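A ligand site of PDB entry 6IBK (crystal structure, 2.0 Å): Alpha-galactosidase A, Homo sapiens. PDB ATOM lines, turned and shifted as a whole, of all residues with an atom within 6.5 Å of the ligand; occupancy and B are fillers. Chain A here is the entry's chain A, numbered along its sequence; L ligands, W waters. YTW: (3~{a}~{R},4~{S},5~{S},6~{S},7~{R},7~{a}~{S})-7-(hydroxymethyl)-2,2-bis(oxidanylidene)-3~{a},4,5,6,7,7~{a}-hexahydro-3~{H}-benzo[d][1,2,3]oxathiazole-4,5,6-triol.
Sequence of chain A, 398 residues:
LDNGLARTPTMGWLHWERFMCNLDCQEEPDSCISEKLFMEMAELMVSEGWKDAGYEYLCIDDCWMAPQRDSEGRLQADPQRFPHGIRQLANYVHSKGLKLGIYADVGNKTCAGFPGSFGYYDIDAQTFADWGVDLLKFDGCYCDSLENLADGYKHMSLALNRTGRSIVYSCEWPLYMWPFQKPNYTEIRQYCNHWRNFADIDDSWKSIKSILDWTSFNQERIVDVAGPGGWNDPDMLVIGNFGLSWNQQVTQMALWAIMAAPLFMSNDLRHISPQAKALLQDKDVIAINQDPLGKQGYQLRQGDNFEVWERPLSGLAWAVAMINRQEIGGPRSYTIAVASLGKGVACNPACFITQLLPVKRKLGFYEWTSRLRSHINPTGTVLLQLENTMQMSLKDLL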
ATOM      1  N   LEU A  14     -28.384  21.521 -18.130  1.00  0.00           N
ATOM      2  CA  LEU A  14     -27.308  20.665 -17.596  1.00  0.00           C
ATOM      3  C   LEU A  14     -27.487  19.270 -18.209  1.00  0.00           C
ATOM      4  O   LEU A  14     -28.612  18.765 -18.240  1.00  0.00           O
ATOM      5  CB  LEU A  14     -27.446  20.701 -16.070  1.00  0.00           C
ATOM      6  CG  LEU A  14     -26.440  19.900 -15.256  1.00  0.00           C
ATOM      7  CD1 LEU A  14     -25.022  20.422 -15.474  1.00  0.00           C
ATOM      8  CD2 LEU A  14     -26.806  19.968 -13.790  1.00  0.00           C
ATOM      9  N   TRP A  16     -26.664  16.227 -17.354  1.00  0.00           N
ATOM     10  CA  TRP A  16     -26.468  14.929 -16.627  1.00  0.00           C
ATOM     11  C   TRP A  16     -27.641  13.966 -16.827  1.00  0.00           C
ATOM     12  O   TRP A  16     -27.402  12.825 -17.203  1.00  0.00           O
ATOM     13  CB  TRP A  16     -26.222  15.101 -15.140  1.00  0.00           C
ATOM     14  CG  TRP A  16     -25.943  13.782 -14.503  1.00  0.00           C
ATOM     15  CD1 TRP A  16     -26.717  13.120 -13.593  1.00  0.00           C
ATOM     16  CD2 TRP A  16     -24.826  12.920 -14.785  1.00  0.00           C
ATOM     17  NE1 TRP A  16     -26.136  11.920 -13.265  1.00  0.00           N
ATOM     18  CE2 TRP A  16     -24.990  11.771 -13.987  1.00  0.00           C
ATOM     19  CE3 TRP A  16     -23.737  12.995 -15.646  1.00  0.00           C
ATOM     20  CZ2 TRP A  16     -24.077  10.714 -14.020  1.00  0.00           C
ATOM     21  CZ3 TRP A  16     -22.829  11.960 -15.658  1.00  0.00           C
ATOM     22  CH2 TRP A  16     -22.999  10.841 -14.846  1.00  0.00           C
ATOM     23  N   MET A  20     -26.058  11.826 -19.336  1.00  0.00           N
ATOM     24  CA  MET A  20     -25.298  10.958 -18.381  1.00  0.00           C
ATOM     25  C   MET A  20     -23.811  10.935 -18.789  1.00  0.00           C
ATOM     26  O   MET A  20     -23.296  11.998 -19.152  1.00  0.00           O
ATOM     27  CB  MET A  20     -25.886   9.540 -18.348  1.00  0.00           C
ATOM     28  CG  MET A  20     -27.399   9.506 -18.054  1.00  0.00           C
ATOM     29  SD  MET A  20     -27.829   8.285 -16.792  1.00  0.00           S
ATOM     30  CE  MET A  20     -27.090   9.148 -15.412  1.00  0.00           C
ATOM     31  N   ASP A  61     -21.725  18.626 -17.050  1.00  0.00           N
ATOM     32  CA  ASP A  61     -21.669  17.812 -15.809  1.00  0.00           C
ATOM     33  C   ASP A  61     -20.438  16.923 -15.947  1.00  0.00           C
ATOM     34  O   ASP A  61     -19.586  17.266 -16.751  1.00  0.00           O
ATOM     35  CB  ASP A  61     -22.991  17.079 -15.554  1.00  0.00           C
ATOM     36  CG  ASP A  61     -23.288  16.879 -14.071  1.00  0.00           C
ATOM     37  OD1 ASP A  61     -24.108  17.667 -13.510  1.00  0.00           O
ATOM     38  OD2 ASP A  61     -22.705  15.952 -13.486  1.00  0.00           O
ATOM     39  N   ASP A  62     -20.380  15.810 -15.216  1.00  0.00           N
ATOM     40  CA  ASP A  62     -19.206  14.893 -15.151  1.00  0.00           C
ATOM     41  C   ASP A  62     -18.938  14.306 -16.545  1.00  0.00           C
ATOM     42  O   ASP A  62     -19.806  14.440 -17.455  1.00  0.00           O
ATOM     43  CB  ASP A  62     -19.495  13.819 -14.097  1.00  0.00           C
ATOM     44  CG  ASP A  62     -18.288  13.082 -13.579  1.00  0.00           C
ATOM     45  OD1 ASP A  62     -17.196  13.300 -14.125  1.00  0.00           O
ATOM     46  OD2 ASP A  62     -18.477  12.268 -12.653  1.00  0.00           O
ATOM     47  N   CYS A  63     -17.739  13.733 -16.719  1.00  0.00           N
ATOM     48  CA  CYS A  63     -17.306  12.968 -17.913  1.00  0.00           C
ATOM     49  C   CYS A  63     -16.905  13.883 -19.091  1.00  0.00           C
ATOM     50  O   CYS A  63     -16.936  13.408 -20.229  1.00  0.00           O
ATOM     51  CB  CYS A  63     -18.384  11.961 -18.321  1.00  0.00           C
ATOM     52  SG  CYS A  63     -18.814  10.802 -16.975  1.00  0.00           S
ATOM     53  N   TYR A 103     -18.068  21.178 -14.257  1.00  0.00           N
ATOM     54  CA  TYR A 103     -18.208  20.266 -13.103  1.00  0.00           C
ATOM     55  C   TYR A 103     -16.810  19.893 -12.639  1.00  0.00           C
ATOM     56  O   TYR A 103     -15.968  19.755 -13.532  1.00  0.00           O
ATOM     57  CB  TYR A 103     -18.975  19.016 -13.521  1.00  0.00           C
ATOM     58  CG  TYR A 103     -18.962  17.834 -12.572  1.00  0.00           C
ATOM     59  CD1 TYR A 103     -17.863  17.004 -12.481  1.00  0.00           C
ATOM     60  CD2 TYR A 103     -20.070  17.504 -11.812  1.00  0.00           C
ATOM     61  CE1 TYR A 103     -17.840  15.907 -11.634  1.00  0.00           C
ATOM     62  CE2 TYR A 103     -20.079  16.393 -10.972  1.00  0.00           C
ATOM     63  CZ  TYR A 103     -18.949  15.598 -10.883  1.00  0.00           C
ATOM     64  OH  TYR A 103     -18.911  14.506 -10.062  1.00  0.00           O
ATOM     65  N   THR A 110     -13.691  12.408  -9.481  1.00  0.00           N
ATOM     66  CA  THR A 110     -15.122  12.719  -9.723  1.00  0.00           C
ATOM     67  C   THR A 110     -15.938  11.444  -9.488  1.00  0.00           C
ATOM     68  O   THR A 110     -15.334  10.348  -9.384  1.00  0.00           O
ATOM     69  CB  THR A 110     -15.355  13.247 -11.130  1.00  0.00           C
ATOM     70  OG1 THR A 110     -15.220  12.136 -12.015  1.00  0.00           O
ATOM     71  CG2 THR A 110     -14.401  14.363 -11.509  1.00  0.00           C
ATOM     72  N   CYS A 111     -17.257  11.548  -9.437  1.00  0.00           N
ATOM     73  CA  CYS A 111     -18.094  10.352  -9.166  1.00  0.00           C
ATOM     74  C   CYS A 111     -17.907   9.324 -10.287  1.00  0.00           C
ATOM     75  O   CYS A 111     -17.900   8.127  -9.960  1.00  0.00           O
ATOM     76  CB  CYS A 111     -19.557  10.716  -8.961  1.00  0.00           C
ATOM     77  SG  CYS A 111     -19.784  11.788  -7.522  1.00  0.00           S
ATOM     78  N   ALA A 112     -17.694   9.747 -11.526  1.00  0.00           N
ATOM     79  CA  ALA A 112     -17.487   8.803 -12.657  1.00  0.00           C
ATOM     80  C   ALA A 112     -15.994   8.396 -12.771  1.00  0.00           C
ATOM     81  O   ALA A 112     -15.658   7.648 -13.712  1.00  0.00           O
ATOM     82  CB  ALA A 112     -18.026   9.399 -13.927  1.00  0.00           C
ATOM     83  N   LYS A 137     -20.222  23.519 -10.841  1.00  0.00           N
ATOM     84  CA  LYS A 137     -20.916  22.511  -9.998  1.00  0.00           C
ATOM     85  C   LYS A 137     -19.829  21.648  -9.365  1.00  0.00           C
ATOM     86  O   LYS A 137     -19.082  21.023 -10.131  1.00  0.00           O
ATOM     87  CB  LYS A 137     -21.863  21.665 -10.845  1.00  0.00           C
ATOM     88  CG  LYS A 137     -22.539  20.530 -10.092  1.00  0.00           C
ATOM     89  CD  LYS A 137     -23.470  19.671 -10.913  1.00  0.00           C
ATOM     90  CE  LYS A 137     -23.893  18.422 -10.166  1.00  0.00           C
ATOM     91  NZ  LYS A 137     -24.948  17.682 -10.909  1.00  0.00           N
ATOM     92  N   ASP A 139     -18.985  18.581  -6.906  1.00  0.00           N
ATOM     93  CA  ASP A 139     -19.511  17.312  -6.345  1.00  0.00           C
ATOM     94  C   ASP A 139     -18.606  16.840  -5.189  1.00  0.00           C
ATOM     95  O   ASP A 139     -17.498  17.367  -5.054  1.00  0.00           O
ATOM     96  CB  ASP A 139     -19.644  16.292  -7.474  1.00  0.00           C
ATOM     97  CG  ASP A 139     -20.618  15.159  -7.228  1.00  0.00           C
ATOM     98  OD1 ASP A 139     -21.059  14.959  -6.068  1.00  0.00           O
ATOM     99  OD2 ASP A 139     -20.924  14.456  -8.201  1.00  0.00           O
ATOM    100  N   CYS A 141     -17.851  13.308  -4.226  1.00  0.00           N
ATOM    101  CA  CYS A 141     -17.400  11.881  -4.224  1.00  0.00           C
ATOM    102  C   CYS A 141     -15.904  11.777  -3.851  1.00  0.00           C
ATOM    103  O   CYS A 141     -15.125  12.738  -4.129  1.00  0.00           O
ATOM    104  CB  CYS A 141     -17.623  11.187  -5.558  1.00  0.00           C
ATOM    105  SG  CYS A 141     -19.336  10.680  -5.878  1.00  0.00           S
ATOM    106  N   GLU A 172     -22.396  20.474  -3.524  1.00  0.00           N
ATOM    107  CA  GLU A 172     -23.152  19.266  -3.118  1.00  0.00           C
ATOM    108  C   GLU A 172     -22.848  18.934  -1.646  1.00  0.00           C
ATOM    109  O   GLU A 172     -23.258  17.849  -1.174  1.00  0.00           O
ATOM    110  CB  GLU A 172     -22.868  18.100  -4.070  1.00  0.00           C
ATOM    111  CG  GLU A 172     -23.326  18.373  -5.496  1.00  0.00           C
ATOM    112  CD  GLU A 172     -23.705  17.130  -6.285  1.00  0.00           C
ATOM    113  OE1 GLU A 172     -24.442  16.265  -5.740  1.00  0.00           O
ATOM    114  OE2 GLU A 172     -23.251  17.039  -7.450  1.00  0.00           O
ATOM    115  N   LEU A 175     -25.667  17.429   0.830  1.00  0.00           N
ATOM    116  CA  LEU A 175     -25.954  16.045   0.371  1.00  0.00           C
ATOM    117  C   LEU A 175     -24.927  15.074   0.975  1.00  0.00           C
ATOM    118  O   LEU A 175     -25.355  14.056   1.497  1.00  0.00           O
ATOM    119  CB  LEU A 175     -25.920  15.967  -1.157  1.00  0.00           C
ATOM    120  CG  LEU A 175     -26.149  14.594  -1.768  1.00  0.00           C
ATOM    121  CD1 LEU A 175     -27.484  14.013  -1.266  1.00  0.00           C
ATOM    122  CD2 LEU A 175     -26.120  14.673  -3.291  1.00  0.00           C
ATOM    123  N   TYR A 176     -23.620  15.370   0.877  1.00  0.00           N
ATOM    124  CA  TYR A 176     -22.538  14.420   1.271  1.00  0.00           C
ATOM    125  C   TYR A 176     -22.340  14.375   2.791  1.00  0.00           C
ATOM    126  O   TYR A 176     -21.903  13.343   3.285  1.00  0.00           O
ATOM    127  CB  TYR A 176     -21.247  14.713   0.508  1.00  0.00           C
ATOM    128  CG  TYR A 176     -21.340  14.205  -0.904  1.00  0.00           C
ATOM    129  CD1 TYR A 176     -21.063  12.883  -1.233  1.00  0.00           C
ATOM    130  CD2 TYR A 176     -21.843  15.025  -1.899  1.00  0.00           C
ATOM    131  CE1 TYR A 176     -21.202  12.426  -2.537  1.00  0.00           C
ATOM    132  CE2 TYR A 176     -21.982  14.582  -3.204  1.00  0.00           C
ATOM    133  CZ  TYR A 176     -21.663  13.288  -3.530  1.00  0.00           C
ATOM    134  OH  TYR A 176     -21.780  12.894  -4.835  1.00  0.00           O
ATOM    135  N   ARG A 196     -27.063  21.256  -3.291  1.00  0.00           N
ATOM    136  CA  ARG A 196     -27.856  20.027  -3.413  1.00  0.00           C
ATOM    137  C   ARG A 196     -28.080  19.503  -1.990  1.00  0.00           C
ATOM    138  O   ARG A 196     -27.128  19.381  -1.209  1.00  0.00           O
ATOM    139  CB  ARG A 196     -27.138  19.049  -4.367  1.00  0.00           C
ATOM    140  CG  ARG A 196     -27.267  19.415  -5.845  1.00  0.00           C
ATOM    141  CD  ARG A 196     -28.578  18.929  -6.430  1.00  0.00           C
ATOM    142  NE  ARG A 196     -28.724  17.513  -6.120  1.00  0.00           N
ATOM    143  CZ  ARG A 196     -28.133  16.515  -6.767  1.00  0.00           C
ATOM    144  NH1 ARG A 196     -27.363  16.741  -7.836  1.00  0.00           N
ATOM    145  NH2 ARG A 196     -28.297  15.284  -6.327  1.00  0.00           N
ATOM    146  N   PHE A 198     -30.273  16.604  -1.566  1.00  0.00           N
ATOM    147  CA  PHE A 198     -30.926  15.270  -1.648  1.00  0.00           C
ATOM    148  C   PHE A 198     -30.439  14.495  -2.875  1.00  0.00           C
ATOM    149  O   PHE A 198     -29.756  15.053  -3.765  1.00  0.00           O
ATOM    150  CB  PHE A 198     -32.453  15.483  -1.578  1.00  0.00           C
ATOM    151  CG  PHE A 198     -33.257  14.209  -1.426  1.00  0.00           C
ATOM    152  CD1 PHE A 198     -33.229  13.490  -0.229  1.00  0.00           C
ATOM    153  CD2 PHE A 198     -34.017  13.708  -2.478  1.00  0.00           C
ATOM    154  CE1 PHE A 198     -33.952  12.306  -0.094  1.00  0.00           C
ATOM    155  CE2 PHE A 198     -34.721  12.524  -2.347  1.00  0.00           C
ATOM    156  CZ  PHE A 198     -34.701  11.842  -1.143  1.00  0.00           C
ATOM    157  N   ALA A 199     -30.756  13.199  -2.883  1.00  0.00           N
ATOM    158  CA  ALA A 199     -30.421  12.163  -3.891  1.00  0.00           C
ATOM    159  C   ALA A 199     -30.779  12.656  -5.304  1.00  0.00           C
ATOM    160  O   ALA A 199     -31.760  13.389  -5.451  1.00  0.00           O
ATOM    161  CB  ALA A 199     -31.154  10.880  -3.559  1.00  0.00           C
ATOM    162  N   ASP A 200     -29.938  12.315  -6.270  1.00  0.00           N
ATOM    163  CA  ASP A 200     -30.061  12.626  -7.717  1.00  0.00           C
ATOM    164  C   ASP A 200     -31.510  12.413  -8.166  1.00  0.00           C
ATOM    165  O   ASP A 200     -32.123  11.391  -7.828  1.00  0.00           O
ATOM    166  CB  ASP A 200     -29.124  11.742  -8.523  1.00  0.00           C
ATOM    167  CG  ASP A 200     -27.651  12.061  -8.296  1.00  0.00           C
ATOM    168  OD1 ASP A 200     -27.362  12.893  -7.408  1.00  0.00           O
ATOM    169  OD2 ASP A 200     -26.812  11.474  -9.021  1.00  0.00           O
ATOM    170  N   ASP A 235     -32.511  19.651  -7.529  1.00  0.00           N
ATOM    171  CA  ASP A 235     -31.957  18.982  -8.743  1.00  0.00           C
ATOM    172  C   ASP A 235     -32.783  19.355  -9.991  1.00  0.00           C
ATOM    173  O   ASP A 235     -33.747  20.148  -9.885  1.00  0.00           O
ATOM    174  CB  ASP A 235     -31.757  17.465  -8.525  1.00  0.00           C
ATOM    175  CG  ASP A 235     -30.580  16.872  -9.297  1.00  0.00           C
ATOM    176  OD1 ASP A 235     -29.916  17.626 -10.021  1.00  0.00           O
ATOM    177  OD2 ASP A 235     -30.359  15.638  -9.198  1.00  0.00           O
ATOM    178  N   MET A 236     -32.405  18.792 -11.128  1.00  0.00           N
ATOM    179  CA  MET A 236     -32.766  19.224 -12.500  1.00  0.00           C
ATOM    180  C   MET A 236     -34.283  19.059 -12.756  1.00  0.00           C
ATOM    181  O   MET A 236     -34.938  18.176 -12.163  1.00  0.00           O
ATOM    182  CB  MET A 236     -31.975  18.383 -13.508  1.00  0.00           C
ATOM    183  CG  MET A 236     -30.473  18.621 -13.414  1.00  0.00           C
ATOM    184  SD  MET A 236     -29.495  17.351 -14.275  1.00  0.00           S
ATOM    185  CE  MET A 236     -29.196  16.208 -12.929  1.00  0.00           C
HETATM  186  O1  YTW L   1     -24.399   9.638  -9.922  1.00  0.00           O
HETATM  187  S1  YTW L   1     -23.637  10.270  -8.916  1.00  0.00           S
HETATM  188  O2  YTW L   1     -23.137   9.483  -7.850  1.00  0.00           O
HETATM  189  N1  YTW L   1     -24.387  11.603  -8.372  1.00  0.00           N
HETATM  190  C1  YTW L   1     -23.464  12.734  -8.432  1.00  0.00           C
HETATM  191  C2  YTW L   1     -22.552  12.404  -9.633  1.00  0.00           C
HETATM  192  O3  YTW L   1     -22.384  10.983  -9.568  1.00  0.00           O
HETATM  193  C3  YTW L   1     -23.091  12.751 -11.017  1.00  0.00           C
HETATM  194  C4  YTW L   1     -21.935  12.874 -11.999  1.00  0.00           C
HETATM  195  O4  YTW L   1     -21.012  11.802 -11.845  1.00  0.00           O
HETATM  196  C5  YTW L   1     -24.024  13.971 -11.092  1.00  0.00           C
HETATM  197  O5  YTW L   1     -23.268  15.186 -11.084  1.00  0.00           O
HETATM  198  C6  YTW L   1     -24.994  14.021  -9.939  1.00  0.00           C
HETATM  199  O6  YTW L   1     -25.793  15.202 -10.049  1.00  0.00           O
HETATM  200  C7  YTW L   1     -24.227  14.044  -8.624  1.00  0.00           C
HETATM  201  O7  YTW L   1     -25.100  14.226  -7.509  1.00  0.00           O
HETATM  202  O   HOH W   1     -28.444  14.443 -10.414  1.00  0.00           O
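OD2 of Asp 62 lies within hydrogen-bond range of O4 of the ligand (2.7 Å).
The side-chain amino group (NZ) of Lys 137 is in hydrogen-bond range of an oxygen (O6) of the ligand, 2.8 Å away.
The side-chain carboxylate (OE1) of Glu 172 sits at hydrogen-bond distance from an oxygen (O7) of the ligand (2.8 Å).
The side-chain carboxylate (OD2) of Asp 61 lies within hydrogen-bond range of an oxygen (O5) of the ligand, 2.6 Å away.
OD2 of Asp 200 sits at hydrogen-bond distance from N1 of the ligand (2.5 Å).
The guanidinium group (NH1) of Arg 196 sits at hydrogen-bond distance from an oxygen (O6) of the ligand.
The backbone NH (N) of Ala 112 lies within hydrogen-bond range of the side-chain carboxylate (OD2) of Asp 62 (2.9 Å).
The guanidinium group of Arg 196 is in salt-bridge range of the side-chain carboxylate of Asp 200 (2.8 Å).
The side-chain carboxylate of Asp 62 sits at hydrogen-bond distance from the side-chain hydroxyl of Thr 110 (3.1 Å).
OD2 of Asp 62 is in hydrogen-bond range of OH of Tyr 103.
OD1 of Asp 61 is in salt-bridge range of NZ of Lys 137.
The side-chain amino group of Lys 137 lies within salt-bridge range of the side-chain carboxylate of Glu 172, at 3.9 Å.
The backbone NH (N) of Ala 112 sits close to the side-chain hydroxyl (OG1) of Thr 110 (3.5 Å).
The guanidinium group (NH1) of Arg 196 is in salt-bridge range of the side-chain carboxylate (OD2) of Asp 235 (3.5 Å).
SG of Cys 111 sits close to O3 of the ligand, 3.4 Å away.
Merely in contact with the ligand: Trp 16 (3.7 Å), Tyr 103 (3.4 Å), Ala 112 (3.9 Å), Asp 139 (3.0 Å) and Tyr 176 (3.97 Å).
Hydrophobic or aromatic side chains that line the ligand: Trp 16 and Tyr 103.
Water W1 bridges OD2 of Asp 235 (2.6 Å) and O6 of the ligand (2.8 Å).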
